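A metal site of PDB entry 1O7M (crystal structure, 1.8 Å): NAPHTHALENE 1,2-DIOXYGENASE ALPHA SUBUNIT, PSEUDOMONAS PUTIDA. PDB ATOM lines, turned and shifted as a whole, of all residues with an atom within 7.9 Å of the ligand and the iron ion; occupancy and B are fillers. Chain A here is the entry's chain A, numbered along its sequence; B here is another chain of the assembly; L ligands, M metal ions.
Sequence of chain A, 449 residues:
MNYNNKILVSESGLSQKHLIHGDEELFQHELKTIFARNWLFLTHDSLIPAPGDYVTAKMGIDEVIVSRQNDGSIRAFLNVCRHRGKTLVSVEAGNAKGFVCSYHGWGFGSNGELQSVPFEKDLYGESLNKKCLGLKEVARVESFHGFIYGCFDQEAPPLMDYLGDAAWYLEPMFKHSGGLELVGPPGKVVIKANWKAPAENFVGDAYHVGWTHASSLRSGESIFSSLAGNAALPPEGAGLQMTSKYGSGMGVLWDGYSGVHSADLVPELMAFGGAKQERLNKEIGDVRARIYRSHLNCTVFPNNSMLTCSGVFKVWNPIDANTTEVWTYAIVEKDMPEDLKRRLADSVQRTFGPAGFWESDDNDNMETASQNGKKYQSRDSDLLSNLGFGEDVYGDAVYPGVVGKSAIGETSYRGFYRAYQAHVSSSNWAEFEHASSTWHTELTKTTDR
The side-chain amide nitrogen of Asn 201 sits close to an oxygen (O2) of the ligand, 3.4 Å away.
OD1 of Asp 361 sits at hydrogen-bond distance from ND1 of His 213 (2.9 Å).
A ring nitrogen (ND1) of His 213 sits close to the backbone carbonyl oxygen (O) of Trp 358.
The side-chain hydroxyl of Tyr 103 of chain B lies within hydrogen-bond range of the side-chain amide oxygen of Asn 201 (3.2 Å).
ND1 of His 208 sits at hydrogen-bond distance from O of Asp 205, 2.8 Å away.
A ring nitrogen (NE2) of His 208 sits close to the side-chain amide oxygen (OD1) of Asn 201, at 3.4 Å.
CZ of Phe 352 touches O1 of the ligand, 3.8 Å away.
Hydrophobic or aromatic side chains within 4 Å of the ligand: His 208, His 213 and Phe 352.
Residues that only touch the iron ion: Asn 201 (3.97 Å).
The nearest printed residue that does not touch the iron ion is Thr 212 (4.7 Å).
The iron ion is bound by a ring nitrogen (NE2) of His 213 (2.0 Å), a ring nitrogen (NE2) of His 208 (2.1 Å), an oxygen (O1) of the ligand (2.1 Å), the side-chain carboxylate (OD2) of Asp 362 (2.2 Å) and the side-chain carboxylate (OD1) of Asp 362 (2.4 Å).
The iron ion has five donor atoms within binding distance.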
ATOM      1  N   PRO A 198      27.539 -17.219  13.374  1.00  0.00           N
ATOM      2  CA  PRO A 198      27.350 -15.764  13.597  1.00  0.00           C
ATOM      3  C   PRO A 198      28.600 -14.975  13.308  1.00  0.00           C
ATOM      4  O   PRO A 198      28.494 -13.859  12.752  1.00  0.00           O
ATOM      5  CB  PRO A 198      26.955 -15.666  15.065  1.00  0.00           C
ATOM      6  CG  PRO A 198      27.368 -16.997  15.696  1.00  0.00           C
ATOM      7  CD  PRO A 198      27.317 -17.990  14.587  1.00  0.00           C
ATOM      8  N   ASN A 201      28.759 -14.293   9.680  1.00  0.00           N
ATOM      9  CA  ASN A 201      27.627 -13.477   9.274  1.00  0.00           C
ATOM     10  C   ASN A 201      27.925 -11.994   9.547  1.00  0.00           C
ATOM     11  O   ASN A 201      27.745 -11.135   8.666  1.00  0.00           O
ATOM     12  CB  ASN A 201      26.341 -13.937   9.967  1.00  0.00           C
ATOM     13  CG  ASN A 201      25.173 -13.048   9.643  1.00  0.00           C
ATOM     14  OD1 ASN A 201      24.284 -13.415   8.894  1.00  0.00           O
ATOM     15  ND2 ASN A 201      25.186 -11.840  10.205  1.00  0.00           N
ATOM     16  N   PHE A 202      28.424 -11.717  10.746  1.00  0.00           N
ATOM     17  CA  PHE A 202      28.790 -10.351  11.149  1.00  0.00           C
ATOM     18  C   PHE A 202      30.038  -9.823  10.436  1.00  0.00           C
ATOM     19  O   PHE A 202      30.131  -8.620  10.175  1.00  0.00           O
ATOM     20  CB  PHE A 202      28.987 -10.234  12.671  1.00  0.00           C
ATOM     21  CG  PHE A 202      27.715 -10.013  13.433  1.00  0.00           C
ATOM     22  CD1 PHE A 202      26.756 -10.991  13.506  1.00  0.00           C
ATOM     23  CD2 PHE A 202      27.486  -8.820  14.104  1.00  0.00           C
ATOM     24  CE1 PHE A 202      25.601 -10.785  14.177  1.00  0.00           C
ATOM     25  CE2 PHE A 202      26.299  -8.635  14.802  1.00  0.00           C
ATOM     26  CZ  PHE A 202      25.364  -9.613  14.823  1.00  0.00           C
ATOM     27  N   ASP A 205      28.636 -10.319   5.901  1.00  0.00           N
ATOM     28  CA  ASP A 205      27.421 -10.681   5.214  1.00  0.00           C
ATOM     29  C   ASP A 205      26.359  -9.592   5.157  1.00  0.00           C
ATOM     30  O   ASP A 205      25.439  -9.532   5.988  1.00  0.00           O
ATOM     31  CB  ASP A 205      26.805 -11.922   5.819  1.00  0.00           C
ATOM     32  CG  ASP A 205      25.838 -12.585   4.878  1.00  0.00           C
ATOM     33  OD1 ASP A 205      25.904 -13.829   4.727  1.00  0.00           O
ATOM     34  OD2 ASP A 205      25.007 -11.886   4.284  1.00  0.00           O
ATOM     35  N   ALA A 206      26.474  -8.727   4.164  1.00  0.00           N
ATOM     36  CA  ALA A 206      25.414  -7.759   3.921  1.00  0.00           C
ATOM     37  C   ALA A 206      24.355  -8.344   2.963  1.00  0.00           C
ATOM     38  O   ALA A 206      23.247  -7.820   2.889  1.00  0.00           O
ATOM     39  CB  ALA A 206      25.981  -6.478   3.376  1.00  0.00           C
ATOM     40  N   HIS A 208      22.592 -10.977   3.120  1.00  0.00           N
ATOM     41  CA  HIS A 208      21.403 -11.577   3.747  1.00  0.00           C
ATOM     42  C   HIS A 208      20.405 -10.548   4.247  1.00  0.00           C
ATOM     43  O   HIS A 208      19.232 -10.844   4.409  1.00  0.00           O
ATOM     44  CB  HIS A 208      21.800 -12.505   4.907  1.00  0.00           C
ATOM     45  CG  HIS A 208      22.046 -11.794   6.195  1.00  0.00           C
ATOM     46  ND1 HIS A 208      23.162 -11.020   6.425  1.00  0.00           N
ATOM     47  CD2 HIS A 208      21.323 -11.756   7.343  1.00  0.00           C
ATOM     48  CE1 HIS A 208      23.103 -10.540   7.662  1.00  0.00           C
ATOM     49  NE2 HIS A 208      21.994 -10.953   8.228  1.00  0.00           N
ATOM     50  N   VAL A 209      20.864  -9.315   4.465  1.00  0.00           N
ATOM     51  CA  VAL A 209      20.044  -8.334   5.167  1.00  0.00           C
ATOM     52  C   VAL A 209      18.632  -8.140   4.598  1.00  0.00           C
ATOM     53  O   VAL A 209      17.641  -8.293   5.298  1.00  0.00           O
ATOM     54  CB  VAL A 209      20.782  -7.017   5.369  1.00  0.00           C
ATOM     55  CG1 VAL A 209      19.877  -5.950   6.033  1.00  0.00           C
ATOM     56  CG2 VAL A 209      22.017  -7.256   6.241  1.00  0.00           C
ATOM     57  N   THR A 212      16.745 -12.014   4.781  1.00  0.00           N
ATOM     58  CA  THR A 212      16.624 -12.518   6.160  1.00  0.00           C
ATOM     59  C   THR A 212      15.869 -11.566   7.055  1.00  0.00           C
ATOM     60  O   THR A 212      14.994 -11.982   7.796  1.00  0.00           O
ATOM     61  CB  THR A 212      18.015 -12.755   6.800  1.00  0.00           C
ATOM     62  OG1 THR A 212      18.633 -13.915   6.221  1.00  0.00           O
ATOM     63  CG2 THR A 212      17.866 -13.083   8.285  1.00  0.00           C
ATOM     64  N   HIS A 213      16.179 -10.270   6.968  1.00  0.00           N
ATOM     65  CA  HIS A 213      15.608  -9.265   7.875  1.00  0.00           C
ATOM     66  C   HIS A 213      14.443  -8.483   7.250  1.00  0.00           C
ATOM     67  O   HIS A 213      14.101  -7.417   7.722  1.00  0.00           O
ATOM     68  CB  HIS A 213      16.686  -8.302   8.357  1.00  0.00           C
ATOM     69  CG  HIS A 213      17.749  -8.947   9.195  1.00  0.00           C
ATOM     70  ND1 HIS A 213      17.470  -9.501  10.436  1.00  0.00           N
ATOM     71  CD2 HIS A 213      19.065  -9.150   8.975  1.00  0.00           C
ATOM     72  CE1 HIS A 213      18.579 -10.015  10.939  1.00  0.00           C
ATOM     73  NE2 HIS A 213      19.561  -9.796  10.078  1.00  0.00           N
ATOM     74  N   VAL A 260      20.301   0.105  12.901  1.00  0.00           N
ATOM     75  CA  VAL A 260      19.074  -0.663  13.015  1.00  0.00           C
ATOM     76  C   VAL A 260      18.043   0.060  13.869  1.00  0.00           C
ATOM     77  O   VAL A 260      16.877  -0.364  13.938  1.00  0.00           O
ATOM     78  CB  VAL A 260      19.358  -2.055  13.607  1.00  0.00           C
ATOM     79  CG1 VAL A 260      20.385  -2.791  12.757  1.00  0.00           C
ATOM     80  CG2 VAL A 260      19.837  -1.937  15.017  1.00  0.00           C
ATOM     81  N   HIS A 295      28.127   2.739   9.260  1.00  0.00           N
ATOM     82  CA  HIS A 295      27.824   1.486   9.961  1.00  0.00           C
ATOM     83  C   HIS A 295      28.832   0.421   9.595  1.00  0.00           C
ATOM     84  O   HIS A 295      28.964   0.072   8.417  1.00  0.00           O
ATOM     85  CB  HIS A 295      26.433   1.057   9.523  1.00  0.00           C
ATOM     86  CG  HIS A 295      25.762   0.065  10.415  1.00  0.00           C
ATOM     87  ND1 HIS A 295      25.759  -1.283  10.136  1.00  0.00           N
ATOM     88  CD2 HIS A 295      25.024   0.225  11.542  1.00  0.00           C
ATOM     89  CE1 HIS A 295      25.069  -1.918  11.078  1.00  0.00           C
ATOM     90  NE2 HIS A 295      24.582  -1.033  11.923  1.00  0.00           N
ATOM     91  N   ASN A 297      29.933  -3.492  10.162  1.00  0.00           N
ATOM     92  CA  ASN A 297      29.617  -4.810  10.669  1.00  0.00           C
ATOM     93  C   ASN A 297      30.961  -5.558  10.672  1.00  0.00           C
ATOM     94  O   ASN A 297      31.507  -5.864   9.628  1.00  0.00           O
ATOM     95  CB  ASN A 297      28.526  -5.555   9.873  1.00  0.00           C
ATOM     96  CG  ASN A 297      28.840  -5.680   8.410  1.00  0.00           C
ATOM     97  OD1 ASN A 297      28.757  -4.710   7.682  1.00  0.00           O
ATOM     98  ND2 ASN A 297      29.136  -6.912   7.948  1.00  0.00           N
ATOM     99  N   LEU A 307      28.374  -4.165  15.559  1.00  0.00           N
ATOM    100  CA  LEU A 307      27.783  -3.254  14.587  1.00  0.00           C
ATOM    101  C   LEU A 307      28.000  -1.875  15.169  1.00  0.00           C
ATOM    102  O   LEU A 307      27.308  -1.498  16.136  1.00  0.00           O
ATOM    103  CB  LEU A 307      26.289  -3.458  14.376  1.00  0.00           C
ATOM    104  CG  LEU A 307      25.822  -4.876  14.062  1.00  0.00           C
ATOM    105  CD1 LEU A 307      24.325  -4.902  13.905  1.00  0.00           C
ATOM    106  CD2 LEU A 307      26.484  -5.398  12.808  1.00  0.00           C
ATOM    107  N   TRP A 316      30.604 -14.583  20.764  1.00  0.00           N
ATOM    108  CA  TRP A 316      30.070 -15.899  20.409  1.00  0.00           C
ATOM    109  C   TRP A 316      30.880 -16.946  21.164  1.00  0.00           C
ATOM    110  O   TRP A 316      31.880 -17.463  20.663  1.00  0.00           O
ATOM    111  CB  TRP A 316      30.160 -16.145  18.914  1.00  0.00           C
ATOM    112  CG  TRP A 316      29.779 -14.956  18.051  1.00  0.00           C
ATOM    113  CD1 TRP A 316      30.628 -14.201  17.285  1.00  0.00           C
ATOM    114  CD2 TRP A 316      28.468 -14.392  17.860  1.00  0.00           C
ATOM    115  NE1 TRP A 316      29.928 -13.205  16.638  1.00  0.00           N
ATOM    116  CE2 TRP A 316      28.613 -13.290  16.985  1.00  0.00           C
ATOM    117  CE3 TRP A 316      27.195 -14.696  18.354  1.00  0.00           C
ATOM    118  CZ2 TRP A 316      27.526 -12.504  16.576  1.00  0.00           C
ATOM    119  CZ3 TRP A 316      26.122 -13.907  17.945  1.00  0.00           C
ATOM    120  CH2 TRP A 316      26.303 -12.831  17.071  1.00  0.00           C
ATOM    121  N   PHE A 352      18.712  -6.670  18.856  1.00  0.00           N
ATOM    122  CA  PHE A 352      19.688  -7.750  18.820  1.00  0.00           C
ATOM    123  C   PHE A 352      19.972  -8.483  20.113  1.00  0.00           C
ATOM    124  O   PHE A 352      20.874  -9.308  20.135  1.00  0.00           O
ATOM    125  CB  PHE A 352      21.019  -7.227  18.241  1.00  0.00           C
ATOM    126  CG  PHE A 352      21.025  -7.174  16.763  1.00  0.00           C
ATOM    127  CD1 PHE A 352      21.382  -8.284  16.034  1.00  0.00           C
ATOM    128  CD2 PHE A 352      20.620  -6.043  16.111  1.00  0.00           C
ATOM    129  CE1 PHE A 352      21.358  -8.246  14.661  1.00  0.00           C
ATOM    130  CE2 PHE A 352      20.575  -5.980  14.746  1.00  0.00           C
ATOM    131  CZ  PHE A 352      20.944  -7.076  14.001  1.00  0.00           C
ATOM    132  N   TRP A 358      15.422  -8.425  15.379  1.00  0.00           N
ATOM    133  CA  TRP A 358      16.320  -8.663  14.235  1.00  0.00           C
ATOM    134  C   TRP A 358      17.124  -9.940  14.453  1.00  0.00           C
ATOM    135  O   TRP A 358      17.243 -10.738  13.523  1.00  0.00           O
ATOM    136  CB  TRP A 358      17.317  -7.523  14.038  1.00  0.00           C
ATOM    137  CG  TRP A 358      16.749  -6.218  13.609  1.00  0.00           C
ATOM    138  CD1 TRP A 358      15.881  -5.444  14.278  1.00  0.00           C
ATOM    139  CD2 TRP A 358      17.092  -5.500  12.428  1.00  0.00           C
ATOM    140  NE1 TRP A 358      15.635  -4.272  13.595  1.00  0.00           N
ATOM    141  CE2 TRP A 358      16.377  -4.294  12.444  1.00  0.00           C
ATOM    142  CE3 TRP A 358      17.937  -5.771  11.355  1.00  0.00           C
ATOM    143  CZ2 TRP A 358      16.461  -3.359  11.419  1.00  0.00           C
ATOM    144  CZ3 TRP A 358      18.038  -4.844  10.347  1.00  0.00           C
ATOM    145  CH2 TRP A 358      17.307  -3.642  10.387  1.00  0.00           C
ATOM    146  N   GLU A 359      17.720 -10.103  15.642  1.00  0.00           N
ATOM    147  CA  GLU A 359      18.487 -11.315  15.999  1.00  0.00           C
ATOM    148  C   GLU A 359      17.655 -12.587  15.680  1.00  0.00           C
ATOM    149  O   GLU A 359      18.171 -13.541  15.092  1.00  0.00           O
ATOM    150  CB  GLU A 359      18.878 -11.268  17.494  1.00  0.00           C
ATOM    151  CG  GLU A 359      19.785 -12.423  17.997  1.00  0.00           C
ATOM    152  CD  GLU A 359      21.287 -12.170  17.919  1.00  0.00           C
ATOM    153  OE1 GLU A 359      21.773 -11.357  17.085  1.00  0.00           O
ATOM    154  OE2 GLU A 359      22.015 -12.839  18.674  1.00  0.00           O
ATOM    155  N   SER A 360      16.374 -12.574  16.031  1.00  0.00           N
ATOM    156  CA  SER A 360      15.494 -13.729  15.803  1.00  0.00           C
ATOM    157  C   SER A 360      15.409 -14.122  14.326  1.00  0.00           C
ATOM    158  O   SER A 360      15.307 -15.303  13.983  1.00  0.00           O
ATOM    159  CB  SER A 360      14.103 -13.493  16.369  1.00  0.00           C
ATOM    160  OG  SER A 360      13.281 -12.749  15.470  1.00  0.00           O
ATOM    161  N   ASP A 361      15.506 -13.145  13.442  1.00  0.00           N
ATOM    162  CA  ASP A 361      15.494 -13.461  12.023  1.00  0.00           C
ATOM    163  C   ASP A 361      16.668 -14.340  11.631  1.00  0.00           C
ATOM    164  O   ASP A 361      16.585 -15.118  10.683  1.00  0.00           O
ATOM    165  CB  ASP A 361      15.598 -12.202  11.167  1.00  0.00           C
ATOM    166  CG  ASP A 361      14.468 -11.213  11.395  1.00  0.00           C
ATOM    167  OD1 ASP A 361      14.715 -10.013  11.136  1.00  0.00           O
ATOM    168  OD2 ASP A 361      13.337 -11.545  11.811  1.00  0.00           O
ATOM    169  N   ASP A 362      17.777 -14.166  12.322  1.00  0.00           N
ATOM    170  CA  ASP A 362      19.019 -14.826  11.967  1.00  0.00           C
ATOM    171  C   ASP A 362      19.121 -16.218  12.549  1.00  0.00           C
ATOM    172  O   ASP A 362      19.872 -17.047  12.017  1.00  0.00           O
ATOM    173  CB  ASP A 362      20.217 -14.031  12.511  1.00  0.00           C
ATOM    174  CG  ASP A 362      20.546 -12.777  11.733  1.00  0.00           C
ATOM    175  OD1 ASP A 362      20.744 -11.707  12.367  1.00  0.00           O
ATOM    176  OD2 ASP A 362      20.752 -12.778  10.510  1.00  0.00           O
ATOM    177  N   ASN A 363      18.416 -16.478  13.665  1.00  0.00           N
ATOM    178  CA  ASN A 363      18.633 -17.741  14.372  1.00  0.00           C
ATOM    179  C   ASN A 363      18.497 -18.994  13.560  1.00  0.00           C
ATOM    180  O   ASN A 363      19.382 -19.848  13.624  1.00  0.00           O
ATOM    181  CB  ASN A 363      17.753 -17.853  15.633  1.00  0.00           C
ATOM    182  CG  ASN A 363      18.441 -18.652  16.735  1.00  0.00           C
ATOM    183  OD1 ASN A 363      19.645 -18.517  16.974  1.00  0.00           O
ATOM    184  ND2 ASN A 363      17.674 -19.509  17.390  1.00  0.00           N
ATOM    185  N   ASN A 365      18.727 -19.490  10.448  1.00  0.00           N
ATOM    186  CA  ASN A 365      19.800 -19.549   9.459  1.00  0.00           C
ATOM    187  C   ASN A 365      21.062 -20.116  10.114  1.00  0.00           C
ATOM    188  O   ASN A 365      21.703 -21.027   9.575  1.00  0.00           O
ATOM    189  CB  ASN A 365      20.117 -18.171   8.896  1.00  0.00           C
ATOM    190  CG  ASN A 365      18.979 -17.575   8.071  1.00  0.00           C
ATOM    191  OD1 ASN A 365      18.131 -18.263   7.568  1.00  0.00           O
ATOM    192  ND2 ASN A 365      19.009 -16.259   7.926  1.00  0.00           N
ATOM    193  N   MET A 366      21.420 -19.564  11.258  1.00  0.00           N
ATOM    194  CA  MET A 366      22.647 -19.968  11.936  1.00  0.00           C
ATOM    195  C   MET A 366      22.534 -21.395  12.447  1.00  0.00           C
ATOM    196  O   MET A 366      23.476 -22.177  12.308  1.00  0.00           O
ATOM    197  CB  MET A 366      22.947 -19.044  13.084  1.00  0.00           C
ATOM    198  CG  MET A 366      23.002 -17.586  12.703  1.00  0.00           C
ATOM    199  SD  MET A 366      24.442 -17.063  11.972  1.00  0.00           S
ATOM    200  CE  MET A 366      24.166 -17.111  10.187  1.00  0.00           C
ATOM    201  N   TYR B 103      17.861 -17.367   3.807  1.00  0.00           N
ATOM    202  CA  TYR B 103      19.069 -16.710   4.274  1.00  0.00           C
ATOM    203  C   TYR B 103      19.433 -15.592   3.293  1.00  0.00           C
ATOM    204  O   TYR B 103      19.289 -14.419   3.627  1.00  0.00           O
ATOM    205  CB  TYR B 103      20.187 -17.746   4.424  1.00  0.00           C
ATOM    206  CG  TYR B 103      21.384 -17.343   5.267  1.00  0.00           C
ATOM    207  CD1 TYR B 103      22.331 -18.283   5.621  1.00  0.00           C
ATOM    208  CD2 TYR B 103      21.571 -16.047   5.682  1.00  0.00           C
ATOM    209  CE1 TYR B 103      23.446 -17.919   6.399  1.00  0.00           C
ATOM    210  CE2 TYR B 103      22.670 -15.668   6.410  1.00  0.00           C
ATOM    211  CZ  TYR B 103      23.600 -16.606   6.781  1.00  0.00           C
ATOM    212  OH  TYR B 103      24.712 -16.217   7.502  1.00  0.00           O
HETATM  213  O1  LIG L   1      21.934  -8.661  10.677  1.00  0.00           O
HETATM  214  O2  LIG L   1      23.101  -9.368  11.157  1.00  0.00           O
HETATM  215 FE    FE M   1      21.387 -10.693  10.265  1.00  0.00          FE
